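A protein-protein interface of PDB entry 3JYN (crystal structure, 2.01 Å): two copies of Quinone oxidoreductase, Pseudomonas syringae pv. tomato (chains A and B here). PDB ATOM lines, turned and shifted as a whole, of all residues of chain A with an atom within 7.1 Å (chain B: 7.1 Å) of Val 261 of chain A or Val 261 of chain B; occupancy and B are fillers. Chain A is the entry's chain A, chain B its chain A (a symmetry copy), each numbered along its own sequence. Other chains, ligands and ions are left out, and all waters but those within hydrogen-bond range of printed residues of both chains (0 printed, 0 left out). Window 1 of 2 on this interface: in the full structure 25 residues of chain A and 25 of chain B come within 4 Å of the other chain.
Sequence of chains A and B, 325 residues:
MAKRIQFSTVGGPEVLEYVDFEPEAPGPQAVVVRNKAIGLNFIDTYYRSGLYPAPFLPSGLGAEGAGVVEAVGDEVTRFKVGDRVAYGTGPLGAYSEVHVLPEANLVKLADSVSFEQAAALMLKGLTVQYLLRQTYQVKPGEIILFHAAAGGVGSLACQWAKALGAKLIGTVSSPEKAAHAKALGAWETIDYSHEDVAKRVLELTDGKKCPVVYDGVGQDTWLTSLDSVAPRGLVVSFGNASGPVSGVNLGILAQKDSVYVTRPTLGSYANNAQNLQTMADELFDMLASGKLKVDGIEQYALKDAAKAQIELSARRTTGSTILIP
The backbone NH (N) of Val 259 of chain B sits at hydrogen-bond distance from the backbone carbonyl oxygen (O) of Leu 253 of chain B (3.1 Å). N of Tyr 260 of chain B sits at hydrogen-bond distance from O of Gly 233 of chain B (2.8 Å). The backbone carbonyl oxygen of Thr 262 of chain B lies within hydrogen-bond range of the backbone NH of Ser 237 of chain B (3.0 Å). The backbone carbonyl oxygen (O) of Ser 237 of chain B sits close to the guanidinium group (NE) of Arg 263 of chain B. The backbone carbonyl oxygen (O) of Val 235 of chain A is in hydrogen-bond range of the backbone NH (N) of Thr 262 of chain A (3.3 Å). The guanidinium group (NE) of Arg 263 of chain A lies close to the backbone carbonyl oxygen (O) of Ser 237 of chain A, at 3.2 Å.
Leu 250 of chain A touches Arg 263 of chain B, and with the chains exchanged Arg 263 of chain A touches Leu 250 of chain B. Leu 253 of chain A touches Arg 263 of chain B, and with the chains exchanged Arg 263 of chain A touches Leu 253 of chain B. Tyr 260 of chain A touches Val 261 of chain B, and with the chains exchanged Val 261 of chain A touches Tyr 260 of chain B. Val 261 of chain A touches its own counterpart, Val 261 of chain B. Of the 24 pairs that touch across the chains among the printed residues, 24 have their exchanged pair printed and touching as well.
Of the 16 printed residues of chain A, 11 touch a printed residue of chain B. Hydrophobic or aromatic side chains of chain A within 4 Å of the printed part of chain B: Trp 222, Leu 234, Val 248, Leu 250, Leu 253, Tyr 260 and Val 261. Of the 16 printed residues of chain B, 11 touch a printed residue of chain A. Printed residues of chain B that touch a printed residue of chain A: Trp 222, Leu 234, Ser 237, Val 248, Leu 250, Leu 253, Val 259, Tyr 260, Val 261, Thr 262 and Arg 263. Hydrophobic or aromatic side chains of chain B within 4 Å of the printed part of chain A: Trp 222, Leu 234, Val 248, Leu 250, Leu 253, Tyr 260 and Val 261. Along chain B the printed residues that touch a printed residue of chain A span positions 222 to 263. Among the printed residues, 24 pairs touch across the chains. Among the printed residues, no Asp or Glu carboxylate lies within 4 Å of a Lys or Arg side-chain nitrogen of the other chain.
The backbone carbonyl oxygen (O) of Val 259 of chain A lies within hydrogen-bond range of the side-chain hydroxyl (OG1) of Thr 262 of chain B (2.8 Å). N of Val 248 of chain A sits at hydrogen-bond distance from O of Val 248 of chain B (3.1 Å). The backbone carbonyl oxygen (O) of Val 261 of chain A sits at hydrogen-bond distance from the backbone NH (N) of Val 261 of chain B, 3.0 Å away. OG1 of Thr 262 of chain A is in hydrogen-bond range of O of Val 259 of chain B (2.8 Å).
Leu 226 of chain A touches none of the printed residues of chain B. Of the printed residues of chain B, Val 261 of chain A touches Leu 253, Tyr 260 and Val 261. Printed residues of chain A within 4 Å of Leu 250 of chain B: Trp 222, Ser 237 and Arg 263. Of the printed residues of chain A, Tyr 260 of chain B touches Leu 234, Val 261 and Thr 262. Val 261 of chain B touches three residues of chain A. Pro 264 of chain B touches none of the printed residues of chain A. The nearest printed residue of chain A that does not touch Tyr 260 of chain B is Tyr 260 of chain A (5.2 Å).
Among the printed residues, merely in contact across the chains: Trp 222 of chain A with Leu 250 of chain B, Leu 234 of chain A with Tyr 260 of chain B, Ser 237 of chain A with Leu 250 of chain B, Leu 250 of chain A with Trp 222 of chain B, Leu 250 of chain A with Ser 237 of chain B, Leu 250 of chain A with Arg 263 of chain B, Leu 253 of chain A with Val 261 of chain B, Leu 253 of chain A with Thr 262 of chain B, Leu 253 of chain A with Arg 263 of chain B, Val 259 of chain A with Arg 263 of chain B, Tyr 260 of chain A with Leu 234 of chain B, Tyr 260 of chain A with Val 261 of chain B, Tyr 260 of chain A with Thr 262 of chain B, Val 261 of chain A with Leu 253 of chain B, Val 261 of chain A with Tyr 260 of chain B, Thr 262 of chain A with Leu 253 of chain B, Thr 262 of chain A with Tyr 260 of chain B, Arg 263 of chain A with Leu 250 of chain B, Arg 263 of chain A with Leu 253 of chain B and Arg 263 of chain A with Val 259 of chain B.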
ATOM      1  N   TRP A 222       0.131  16.649 -15.351  1.00  0.00           N
ATOM      2  CA  TRP A 222       0.037  17.069 -13.952  1.00  0.00           C
ATOM      3  C   TRP A 222      -0.538  18.476 -13.796  1.00  0.00           C
ATOM      4  O   TRP A 222      -1.503  18.666 -13.054  1.00  0.00           O
ATOM      5  CB  TRP A 222       1.410  16.987 -13.276  1.00  0.00           C
ATOM      6  CG  TRP A 222       1.475  17.546 -11.870  1.00  0.00           C
ATOM      7  CD1 TRP A 222       2.303  18.538 -11.430  1.00  0.00           C
ATOM      8  CD2 TRP A 222       0.738  17.102 -10.717  1.00  0.00           C
ATOM      9  NE1 TRP A 222       2.137  18.737 -10.081  1.00  0.00           N
ATOM     10  CE2 TRP A 222       1.183  17.871  -9.616  1.00  0.00           C
ATOM     11  CE3 TRP A 222      -0.250  16.131 -10.506  1.00  0.00           C
ATOM     12  CZ2 TRP A 222       0.675  17.696  -8.324  1.00  0.00           C
ATOM     13  CZ3 TRP A 222      -0.754  15.959  -9.220  1.00  0.00           C
ATOM     14  CH2 TRP A 222      -0.288  16.738  -8.147  1.00  0.00           C
ATOM     15  N   LEU A 226      -4.173  19.686 -12.315  1.00  0.00           N
ATOM     16  CA  LEU A 226      -4.240  20.641 -11.220  1.00  0.00           C
ATOM     17  C   LEU A 226      -5.121  21.825 -11.592  1.00  0.00           C
ATOM     18  O   LEU A 226      -5.785  22.401 -10.727  1.00  0.00           O
ATOM     19  CB  LEU A 226      -2.840  21.143 -10.850  1.00  0.00           C
ATOM     20  CG  LEU A 226      -1.948  20.198 -10.048  1.00  0.00           C
ATOM     21  CD1 LEU A 226      -0.595  20.860  -9.821  1.00  0.00           C
ATOM     22  CD2 LEU A 226      -2.614  19.858  -8.714  1.00  0.00           C
ATOM     23  N   GLY A 233     -10.874  19.861  -4.389  1.00  0.00           N
ATOM     24  CA  GLY A 233     -11.189  18.650  -5.125  1.00  0.00           C
ATOM     25  C   GLY A 233     -10.031  17.674  -5.065  1.00  0.00           C
ATOM     26  O   GLY A 233      -9.018  17.961  -4.438  1.00  0.00           O
ATOM     27  N   LEU A 234     -10.162  16.532  -5.731  1.00  0.00           N
ATOM     28  CA  LEU A 234      -9.105  15.522  -5.692  1.00  0.00           C
ATOM     29  C   LEU A 234      -8.492  15.167  -7.038  1.00  0.00           C
ATOM     30  O   LEU A 234      -9.207  14.977  -8.018  1.00  0.00           O
ATOM     31  CB  LEU A 234      -9.650  14.239  -5.046  1.00  0.00           C
ATOM     32  CG  LEU A 234      -8.796  12.964  -5.091  1.00  0.00           C
ATOM     33  CD1 LEU A 234      -7.662  13.040  -4.072  1.00  0.00           C
ATOM     34  CD2 LEU A 234      -9.692  11.762  -4.795  1.00  0.00           C
ATOM     35  N   VAL A 235      -7.167  15.079  -7.073  1.00  0.00           N
ATOM     36  CA  VAL A 235      -6.449  14.675  -8.276  1.00  0.00           C
ATOM     37  C   VAL A 235      -5.823  13.304  -8.049  1.00  0.00           C
ATOM     38  O   VAL A 235      -4.908  13.159  -7.239  1.00  0.00           O
ATOM     39  CB  VAL A 235      -5.345  15.681  -8.647  1.00  0.00           C
ATOM     40  CG1 VAL A 235      -4.476  15.129  -9.767  1.00  0.00           C
ATOM     41  CG2 VAL A 235      -5.958  17.015  -9.047  1.00  0.00           C
ATOM     42  N   VAL A 236      -6.326  12.299  -8.755  1.00  0.00           N
ATOM     43  CA  VAL A 236      -5.888  10.924  -8.537  1.00  0.00           C
ATOM     44  C   VAL A 236      -4.801  10.574  -9.552  1.00  0.00           C
ATOM     45  O   VAL A 236      -5.084  10.360 -10.730  1.00  0.00           O
ATOM     46  CB  VAL A 236      -7.050   9.909  -8.695  1.00  0.00           C
ATOM     47  CG1 VAL A 236      -6.524   8.480  -8.489  1.00  0.00           C
ATOM     48  CG2 VAL A 236      -8.162  10.221  -7.694  1.00  0.00           C
ATOM     49  N   SER A 237      -3.559  10.528  -9.088  1.00  0.00           N
ATOM     50  CA  SER A 237      -2.441  10.203  -9.959  1.00  0.00           C
ATOM     51  C   SER A 237      -2.158   8.708  -9.832  1.00  0.00           C
ATOM     52  O   SER A 237      -1.411   8.284  -8.958  1.00  0.00           O
ATOM     53  CB  SER A 237      -1.211  11.014  -9.551  1.00  0.00           C
ATOM     54  OG  SER A 237      -0.084  10.647 -10.317  1.00  0.00           O
ATOM     55  N   VAL A 248       7.467  17.993  -6.715  1.00  0.00           N
ATOM     56  CA  VAL A 248       6.350  18.883  -6.426  1.00  0.00           C
ATOM     57  C   VAL A 248       6.449  19.483  -5.030  1.00  0.00           C
ATOM     58  O   VAL A 248       6.910  18.837  -4.089  1.00  0.00           O
ATOM     59  CB  VAL A 248       4.962  18.177  -6.577  1.00  0.00           C
ATOM     60  CG1 VAL A 248       5.065  17.005  -7.534  1.00  0.00           C
ATOM     61  CG2 VAL A 248       4.425  17.752  -5.226  1.00  0.00           C
ATOM     62  N   LEU A 250       4.364  20.894  -1.978  1.00  0.00           N
ATOM     63  CA  LEU A 250       3.000  20.787  -1.483  1.00  0.00           C
ATOM     64  C   LEU A 250       2.300  22.136  -1.552  1.00  0.00           C
ATOM     65  O   LEU A 250       1.073  22.207  -1.559  1.00  0.00           O
ATOM     66  CB  LEU A 250       2.991  20.262  -0.049  1.00  0.00           C
ATOM     67  CG  LEU A 250       3.587  18.869   0.148  1.00  0.00           C
ATOM     68  CD1 LEU A 250       3.280  18.395   1.567  1.00  0.00           C
ATOM     69  CD2 LEU A 250       2.993  17.900  -0.870  1.00  0.00           C
ATOM     70  N   LEU A 253      -0.519  22.745  -4.015  1.00  0.00           N
ATOM     71  CA  LEU A 253      -1.858  22.245  -3.719  1.00  0.00           C
ATOM     72  C   LEU A 253      -2.701  23.380  -3.150  1.00  0.00           C
ATOM     73  O   LEU A 253      -3.899  23.469  -3.408  1.00  0.00           O
ATOM     74  CB  LEU A 253      -1.798  21.095  -2.707  1.00  0.00           C
ATOM     75  CG  LEU A 253      -0.991  19.852  -3.101  1.00  0.00           C
ATOM     76  CD1 LEU A 253      -1.065  18.835  -1.964  1.00  0.00           C
ATOM     77  CD2 LEU A 253      -1.541  19.253  -4.385  1.00  0.00           C
ATOM     78  N   VAL A 259      -6.382  21.759  -2.874  1.00  0.00           N
ATOM     79  CA  VAL A 259      -6.817  20.484  -3.410  1.00  0.00           C
ATOM     80  C   VAL A 259      -6.124  19.313  -2.720  1.00  0.00           C
ATOM     81  O   VAL A 259      -5.223  19.498  -1.888  1.00  0.00           O
ATOM     82  CB  VAL A 259      -6.573  20.410  -4.940  1.00  0.00           C
ATOM     83  CG1 VAL A 259      -7.448  21.442  -5.651  1.00  0.00           C
ATOM     84  CG2 VAL A 259      -5.106  20.659  -5.254  1.00  0.00           C
ATOM     85  N   TYR A 260      -6.584  18.110  -3.042  1.00  0.00           N
ATOM     86  CA  TYR A 260      -6.021  16.883  -2.493  1.00  0.00           C
ATOM     87  C   TYR A 260      -5.396  16.079  -3.629  1.00  0.00           C
ATOM     88  O   TYR A 260      -5.801  16.202  -4.784  1.00  0.00           O
ATOM     89  CB  TYR A 260      -7.106  15.997  -1.870  1.00  0.00           C
ATOM     90  CG  TYR A 260      -7.876  16.573  -0.704  1.00  0.00           C
ATOM     91  CD1 TYR A 260      -8.695  17.695  -0.863  1.00  0.00           C
ATOM     92  CD2 TYR A 260      -7.849  15.947   0.543  1.00  0.00           C
ATOM     93  CE1 TYR A 260      -9.472  18.168   0.186  1.00  0.00           C
ATOM     94  CE2 TYR A 260      -8.627  16.415   1.605  1.00  0.00           C
ATOM     95  CZ  TYR A 260      -9.439  17.524   1.415  1.00  0.00           C
ATOM     96  OH  TYR A 260     -10.236  17.975   2.442  1.00  0.00           O
ATOM     97  N   VAL A 261      -4.424  15.241  -3.296  1.00  0.00           N
ATOM     98  CA  VAL A 261      -3.800  14.391  -4.304  1.00  0.00           C
ATOM     99  C   VAL A 261      -3.463  13.052  -3.664  1.00  0.00           C
ATOM    100  O   VAL A 261      -3.081  12.987  -2.498  1.00  0.00           O
ATOM    101  CB  VAL A 261      -2.504  15.024  -4.879  1.00  0.00           C
ATOM    102  CG1 VAL A 261      -1.488  15.242  -3.772  1.00  0.00           C
ATOM    103  CG2 VAL A 261      -1.920  14.121  -5.977  1.00  0.00           C
ATOM    104  N   THR A 262      -3.636  11.979  -4.425  1.00  0.00           N
ATOM    105  CA  THR A 262      -3.305  10.657  -3.921  1.00  0.00           C
ATOM    106  C   THR A 262      -2.669   9.892  -5.062  1.00  0.00           C
ATOM    107  O   THR A 262      -2.923  10.188  -6.225  1.00  0.00           O
ATOM    108  CB  THR A 262      -4.553   9.888  -3.420  1.00  0.00           C
ATOM    109  OG1 THR A 262      -4.152   8.616  -2.891  1.00  0.00           O
ATOM    110  CG2 THR A 262      -5.548   9.665  -4.557  1.00  0.00           C
ATOM    111  N   ARG A 263      -1.826   8.924  -4.718  1.00  0.00           N
ATOM    112  CA  ARG A 263      -1.156   8.084  -5.703  1.00  0.00           C
ATOM    113  C   ARG A 263      -1.405   6.624  -5.360  1.00  0.00           C
ATOM    114  O   ARG A 263      -0.553   5.956  -4.776  1.00  0.00           O
ATOM    115  CB  ARG A 263       0.344   8.377  -5.729  1.00  0.00           C
ATOM    116  CG  ARG A 263       1.004   8.109  -7.072  1.00  0.00           C
ATOM    117  CD  ARG A 263       0.663   6.721  -7.588  1.00  0.00           C
ATOM    118  NE  ARG A 263       1.242   6.468  -8.904  1.00  0.00           N
ATOM    119  CZ  ARG A 263       1.231   5.287  -9.512  1.00  0.00           C
ATOM    120  NH1 ARG A 263       0.668   4.241  -8.921  1.00  0.00           N
ATOM    121  NH2 ARG A 263       1.783   5.149 -10.709  1.00  0.00           N
ATOM    122  N   PRO A 264      -2.587   6.140  -5.723  1.00  0.00           N
ATOM    123  CA  PRO A 264      -3.026   4.797  -5.354  1.00  0.00           C
ATOM    124  C   PRO A 264      -2.393   3.684  -6.178  1.00  0.00           C
ATOM    125  O   PRO A 264      -1.860   3.910  -7.266  1.00  0.00           O
ATOM    126  CB  PRO A 264      -4.530   4.879  -5.553  1.00  0.00           C
ATOM    127  CG  PRO A 264      -4.622   5.709  -6.805  1.00  0.00           C
ATOM    128  CD  PRO A 264      -3.581   6.799  -6.594  1.00  0.00           C
ATOM    129  N   TRP B 222       7.553  15.766   7.889  1.00  0.00           N
ATOM    130  CA  TRP B 222       6.915  15.164   6.716  1.00  0.00           C
ATOM    131  C   TRP B 222       7.017  13.640   6.706  1.00  0.00           C
ATOM    132  O   TRP B 222       5.999  12.957   6.579  1.00  0.00           O
ATOM    133  CB  TRP B 222       7.518  15.738   5.428  1.00  0.00           C
ATOM    134  CG  TRP B 222       7.052  15.078   4.147  1.00  0.00           C
ATOM    135  CD1 TRP B 222       7.844  14.488   3.203  1.00  0.00           C
ATOM    136  CD2 TRP B 222       5.708  15.006   3.638  1.00  0.00           C
ATOM    137  NE1 TRP B 222       7.086  14.060   2.141  1.00  0.00           N
ATOM    138  CE2 TRP B 222       5.772  14.364   2.380  1.00  0.00           C
ATOM    139  CE3 TRP B 222       4.460  15.422   4.120  1.00  0.00           C
ATOM    140  CZ2 TRP B 222       4.636  14.130   1.597  1.00  0.00           C
ATOM    141  CZ3 TRP B 222       3.330  15.188   3.341  1.00  0.00           C
ATOM    142  CH2 TRP B 222       3.429  14.549   2.093  1.00  0.00           C
ATOM    143  N   LEU B 226       4.099  10.803   7.257  1.00  0.00           N
ATOM    144  CA  LEU B 226       3.873   9.775   6.253  1.00  0.00           C
ATOM    145  C   LEU B 226       3.939   8.389   6.878  1.00  0.00           C
ATOM    146  O   LEU B 226       3.241   7.475   6.435  1.00  0.00           O
ATOM    147  CB  LEU B 226       4.910   9.878   5.127  1.00  0.00           C
ATOM    148  CG  LEU B 226       4.723  10.998   4.107  1.00  0.00           C
ATOM    149  CD1 LEU B 226       5.869  10.957   3.105  1.00  0.00           C
ATOM    150  CD2 LEU B 226       3.379  10.839   3.396  1.00  0.00           C
ATOM    151  N   GLY B 233      -4.945   6.719   4.211  1.00  0.00           N
ATOM    152  CA  GLY B 233      -5.300   7.763   5.154  1.00  0.00           C
ATOM    153  C   GLY B 233      -4.908   9.124   4.614  1.00  0.00           C
ATOM    154  O   GLY B 233      -4.384   9.219   3.511  1.00  0.00           O
ATOM    155  N   LEU B 234      -5.136  10.177   5.392  1.00  0.00           N
ATOM    156  CA  LEU B 234      -4.822  11.528   4.927  1.00  0.00           C
ATOM    157  C   LEU B 234      -3.808  12.287   5.769  1.00  0.00           C
ATOM    158  O   LEU B 234      -3.883  12.280   6.995  1.00  0.00           O
ATOM    159  CB  LEU B 234      -6.114  12.354   4.852  1.00  0.00           C
ATOM    160  CG  LEU B 234      -6.016  13.866   4.601  1.00  0.00           C
ATOM    161  CD1 LEU B 234      -5.705  14.149   3.134  1.00  0.00           C
ATOM    162  CD2 LEU B 234      -7.342  14.517   4.994  1.00  0.00           C
ATOM    163  N   VAL B 235      -2.862  12.938   5.101  1.00  0.00           N
ATOM    164  CA  VAL B 235      -1.869  13.767   5.773  1.00  0.00           C
ATOM    165  C   VAL B 235      -2.123  15.230   5.431  1.00  0.00           C
ATOM    166  O   VAL B 235      -1.954  15.645   4.285  1.00  0.00           O
ATOM    167  CB  VAL B 235      -0.436  13.391   5.358  1.00  0.00           C
ATOM    168  CG1 VAL B 235       0.559  14.406   5.900  1.00  0.00           C
ATOM    169  CG2 VAL B 235      -0.095  11.990   5.842  1.00  0.00           C
ATOM    170  N   VAL B 236      -2.543  16.006   6.423  1.00  0.00           N
ATOM    171  CA  VAL B 236      -2.931  17.394   6.189  1.00  0.00           C
ATOM    172  C   VAL B 236      -1.746  18.308   6.500  1.00  0.00           C
ATOM    173  O   VAL B 236      -1.413  18.535   7.663  1.00  0.00           O
ATOM    174  CB  VAL B 236      -4.126  17.823   7.078  1.00  0.00           C
ATOM    175  CG1 VAL B 236      -4.467  19.298   6.815  1.00  0.00           C
ATOM    176  CG2 VAL B 236      -5.339  16.935   6.797  1.00  0.00           C
ATOM    177  N   SER B 237      -1.111  18.820   5.454  1.00  0.00           N
ATOM    178  CA  SER B 237       0.030  19.706   5.626  1.00  0.00           C
ATOM    179  C   SER B 237      -0.474  21.146   5.567  1.00  0.00           C
ATOM    180  O   SER B 237      -0.579  21.729   4.494  1.00  0.00           O
ATOM    181  CB  SER B 237       1.054  19.454   4.519  1.00  0.00           C
ATOM    182  OG  SER B 237       2.128  20.368   4.603  1.00  0.00           O
ATOM    183  N   VAL B 248       8.843  16.564  -3.421  1.00  0.00           N
ATOM    184  CA  VAL B 248       8.257  15.251  -3.183  1.00  0.00           C
ATOM    185  C   VAL B 248       7.839  14.572  -4.479  1.00  0.00           C
ATOM    186  O   VAL B 248       7.393  15.222  -5.425  1.00  0.00           O
ATOM    187  CB  VAL B 248       7.025  15.307  -2.219  1.00  0.00           C
ATOM    188  CG1 VAL B 248       7.110  16.526  -1.320  1.00  0.00           C
ATOM    189  CG2 VAL B 248       5.729  15.277  -3.002  1.00  0.00           C
ATOM    190  N   LEU B 250       5.293  12.011  -6.097  1.00  0.00           N
ATOM    191  CA  LEU B 250       3.990  11.456  -5.765  1.00  0.00           C
ATOM    192  C   LEU B 250       4.095   9.959  -5.512  1.00  0.00           C
ATOM    193  O   LEU B 250       3.237   9.371  -4.858  1.00  0.00           O
ATOM    194  CB  LEU B 250       2.991  11.731  -6.886  1.00  0.00           C
ATOM    195  CG  LEU B 250       2.721  13.205  -7.184  1.00  0.00           C
ATOM    196  CD1 LEU B 250       1.535  13.308  -8.140  1.00  0.00           C
ATOM    197  CD2 LEU B 250       2.418  13.951  -5.888  1.00  0.00           C
ATOM    198  N   LEU B 253       3.626   8.534  -2.029  1.00  0.00           N
ATOM    199  CA  LEU B 253       2.278   8.367  -1.491  1.00  0.00           C
ATOM    200  C   LEU B 253       1.847   6.915  -1.666  1.00  0.00           C
ATOM    201  O   LEU B 253       1.151   6.356  -0.821  1.00  0.00           O
ATOM    202  CB  LEU B 253       1.286   9.285  -2.216  1.00  0.00           C
ATOM    203  CG  LEU B 253       1.551  10.794  -2.154  1.00  0.00           C
ATOM    204  CD1 LEU B 253       0.452  11.520  -2.927  1.00  0.00           C
ATOM    205  CD2 LEU B 253       1.582  11.265  -0.709  1.00  0.00           C
ATOM    206  N   VAL B 259      -1.674   6.748   0.290  1.00  0.00           N
ATOM    207  CA  VAL B 259      -2.251   7.772   1.140  1.00  0.00           C
ATOM    208  C   VAL B 259      -2.618   9.024   0.348  1.00  0.00           C
ATOM    209  O   VAL B 259      -2.330   9.134  -0.852  1.00  0.00           O
ATOM    210  CB  VAL B 259      -1.286   8.146   2.295  1.00  0.00           C
ATOM    211  CG1 VAL B 259      -1.098   6.943   3.219  1.00  0.00           C
ATOM    212  CG2 VAL B 259       0.057   8.594   1.738  1.00  0.00           C
ATOM    213  N   TYR B 260      -3.297   9.944   1.024  1.00  0.00           N
ATOM    214  CA  TYR B 260      -3.707  11.209   0.427  1.00  0.00           C
ATOM    215  C   TYR B 260      -2.988  12.347   1.147  1.00  0.00           C
ATOM    216  O   TYR B 260      -2.613  12.216   2.311  1.00  0.00           O
ATOM    217  CB  TYR B 260      -5.210  11.452   0.607  1.00  0.00           C
ATOM    218  CG  TYR B 260      -6.147  10.452  -0.030  1.00  0.00           C
ATOM    219  CD1 TYR B 260      -6.178   9.120   0.392  1.00  0.00           C
ATOM    220  CD2 TYR B 260      -7.065  10.858  -1.002  1.00  0.00           C
ATOM    221  CE1 TYR B 260      -7.102   8.224  -0.131  1.00  0.00           C
ATOM    222  CE2 TYR B 260      -7.998   9.965  -1.533  1.00  0.00           C
ATOM    223  CZ  TYR B 260      -8.011   8.650  -1.087  1.00  0.00           C
ATOM    224  OH  TYR B 260      -8.948   7.770  -1.577  1.00  0.00           O
ATOM    225  N   VAL B 261      -2.820  13.468   0.460  1.00  0.00           N
ATOM    226  CA  VAL B 261      -2.190  14.629   1.080  1.00  0.00           C
ATOM    227  C   VAL B 261      -2.862  15.885   0.543  1.00  0.00           C
ATOM    228  O   VAL B 261      -3.237  15.952  -0.626  1.00  0.00           O
ATOM    229  CB  VAL B 261      -0.668  14.696   0.781  1.00  0.00           C
ATOM    230  CG1 VAL B 261      -0.429  14.790  -0.715  1.00  0.00           C
ATOM    231  CG2 VAL B 261      -0.043  15.900   1.504  1.00  0.00           C
ATOM    232  N   THR B 262      -3.040  16.871   1.413  1.00  0.00           N
ATOM    233  CA  THR B 262      -3.637  18.127   0.991  1.00  0.00           C
ATOM    234  C   THR B 262      -2.892  19.235   1.705  1.00  0.00           C
ATOM    235  O   THR B 262      -2.326  19.016   2.772  1.00  0.00           O
ATOM    236  CB  THR B 262      -5.143  18.212   1.344  1.00  0.00           C
ATOM    237  OG1 THR B 262      -5.681  19.450   0.857  1.00  0.00           O
ATOM    238  CG2 THR B 262      -5.355  18.135   2.855  1.00  0.00           C
ATOM    239  N   ARG B 263      -2.878  20.416   1.094  1.00  0.00           N
ATOM    240  CA  ARG B 263      -2.223  21.585   1.670  1.00  0.00           C
ATOM    241  C   ARG B 263      -3.213  22.737   1.710  1.00  0.00           C
ATOM    242  O   ARG B 263      -3.193  23.621   0.856  1.00  0.00           O
ATOM    243  CB  ARG B 263      -0.992  21.969   0.849  1.00  0.00           C
ATOM    244  CG  ARG B 263       0.092  22.671   1.652  1.00  0.00           C
ATOM    245  CD  ARG B 263      -0.475  23.833   2.448  1.00  0.00           C
ATOM    246  NE  ARG B 263       0.543  24.482   3.270  1.00  0.00           N
ATOM    247  CZ  ARG B 263       0.353  25.614   3.939  1.00  0.00           C
ATOM    248  NH1 ARG B 263      -0.821  26.228   3.887  1.00  0.00           N
ATOM    249  NH2 ARG B 263       1.337  26.133   4.661  1.00  0.00           N
ATOM    250  N   PRO B 264      -4.087  22.711   2.710  1.00  0.00           N
ATOM    251  CA  PRO B 264      -5.180  23.673   2.816  1.00  0.00           C
ATOM    252  C   PRO B 264      -4.756  25.048   3.314  1.00  0.00           C
ATOM    253  O   PRO B 264      -3.688  25.220   3.905  1.00  0.00           O
ATOM    254  CB  PRO B 264      -6.132  22.981   3.777  1.00  0.00           C
ATOM    255  CG  PRO B 264      -5.173  22.367   4.761  1.00  0.00           C
ATOM    256  CD  PRO B 264      -4.061  21.811   3.882  1.00  0.00           C
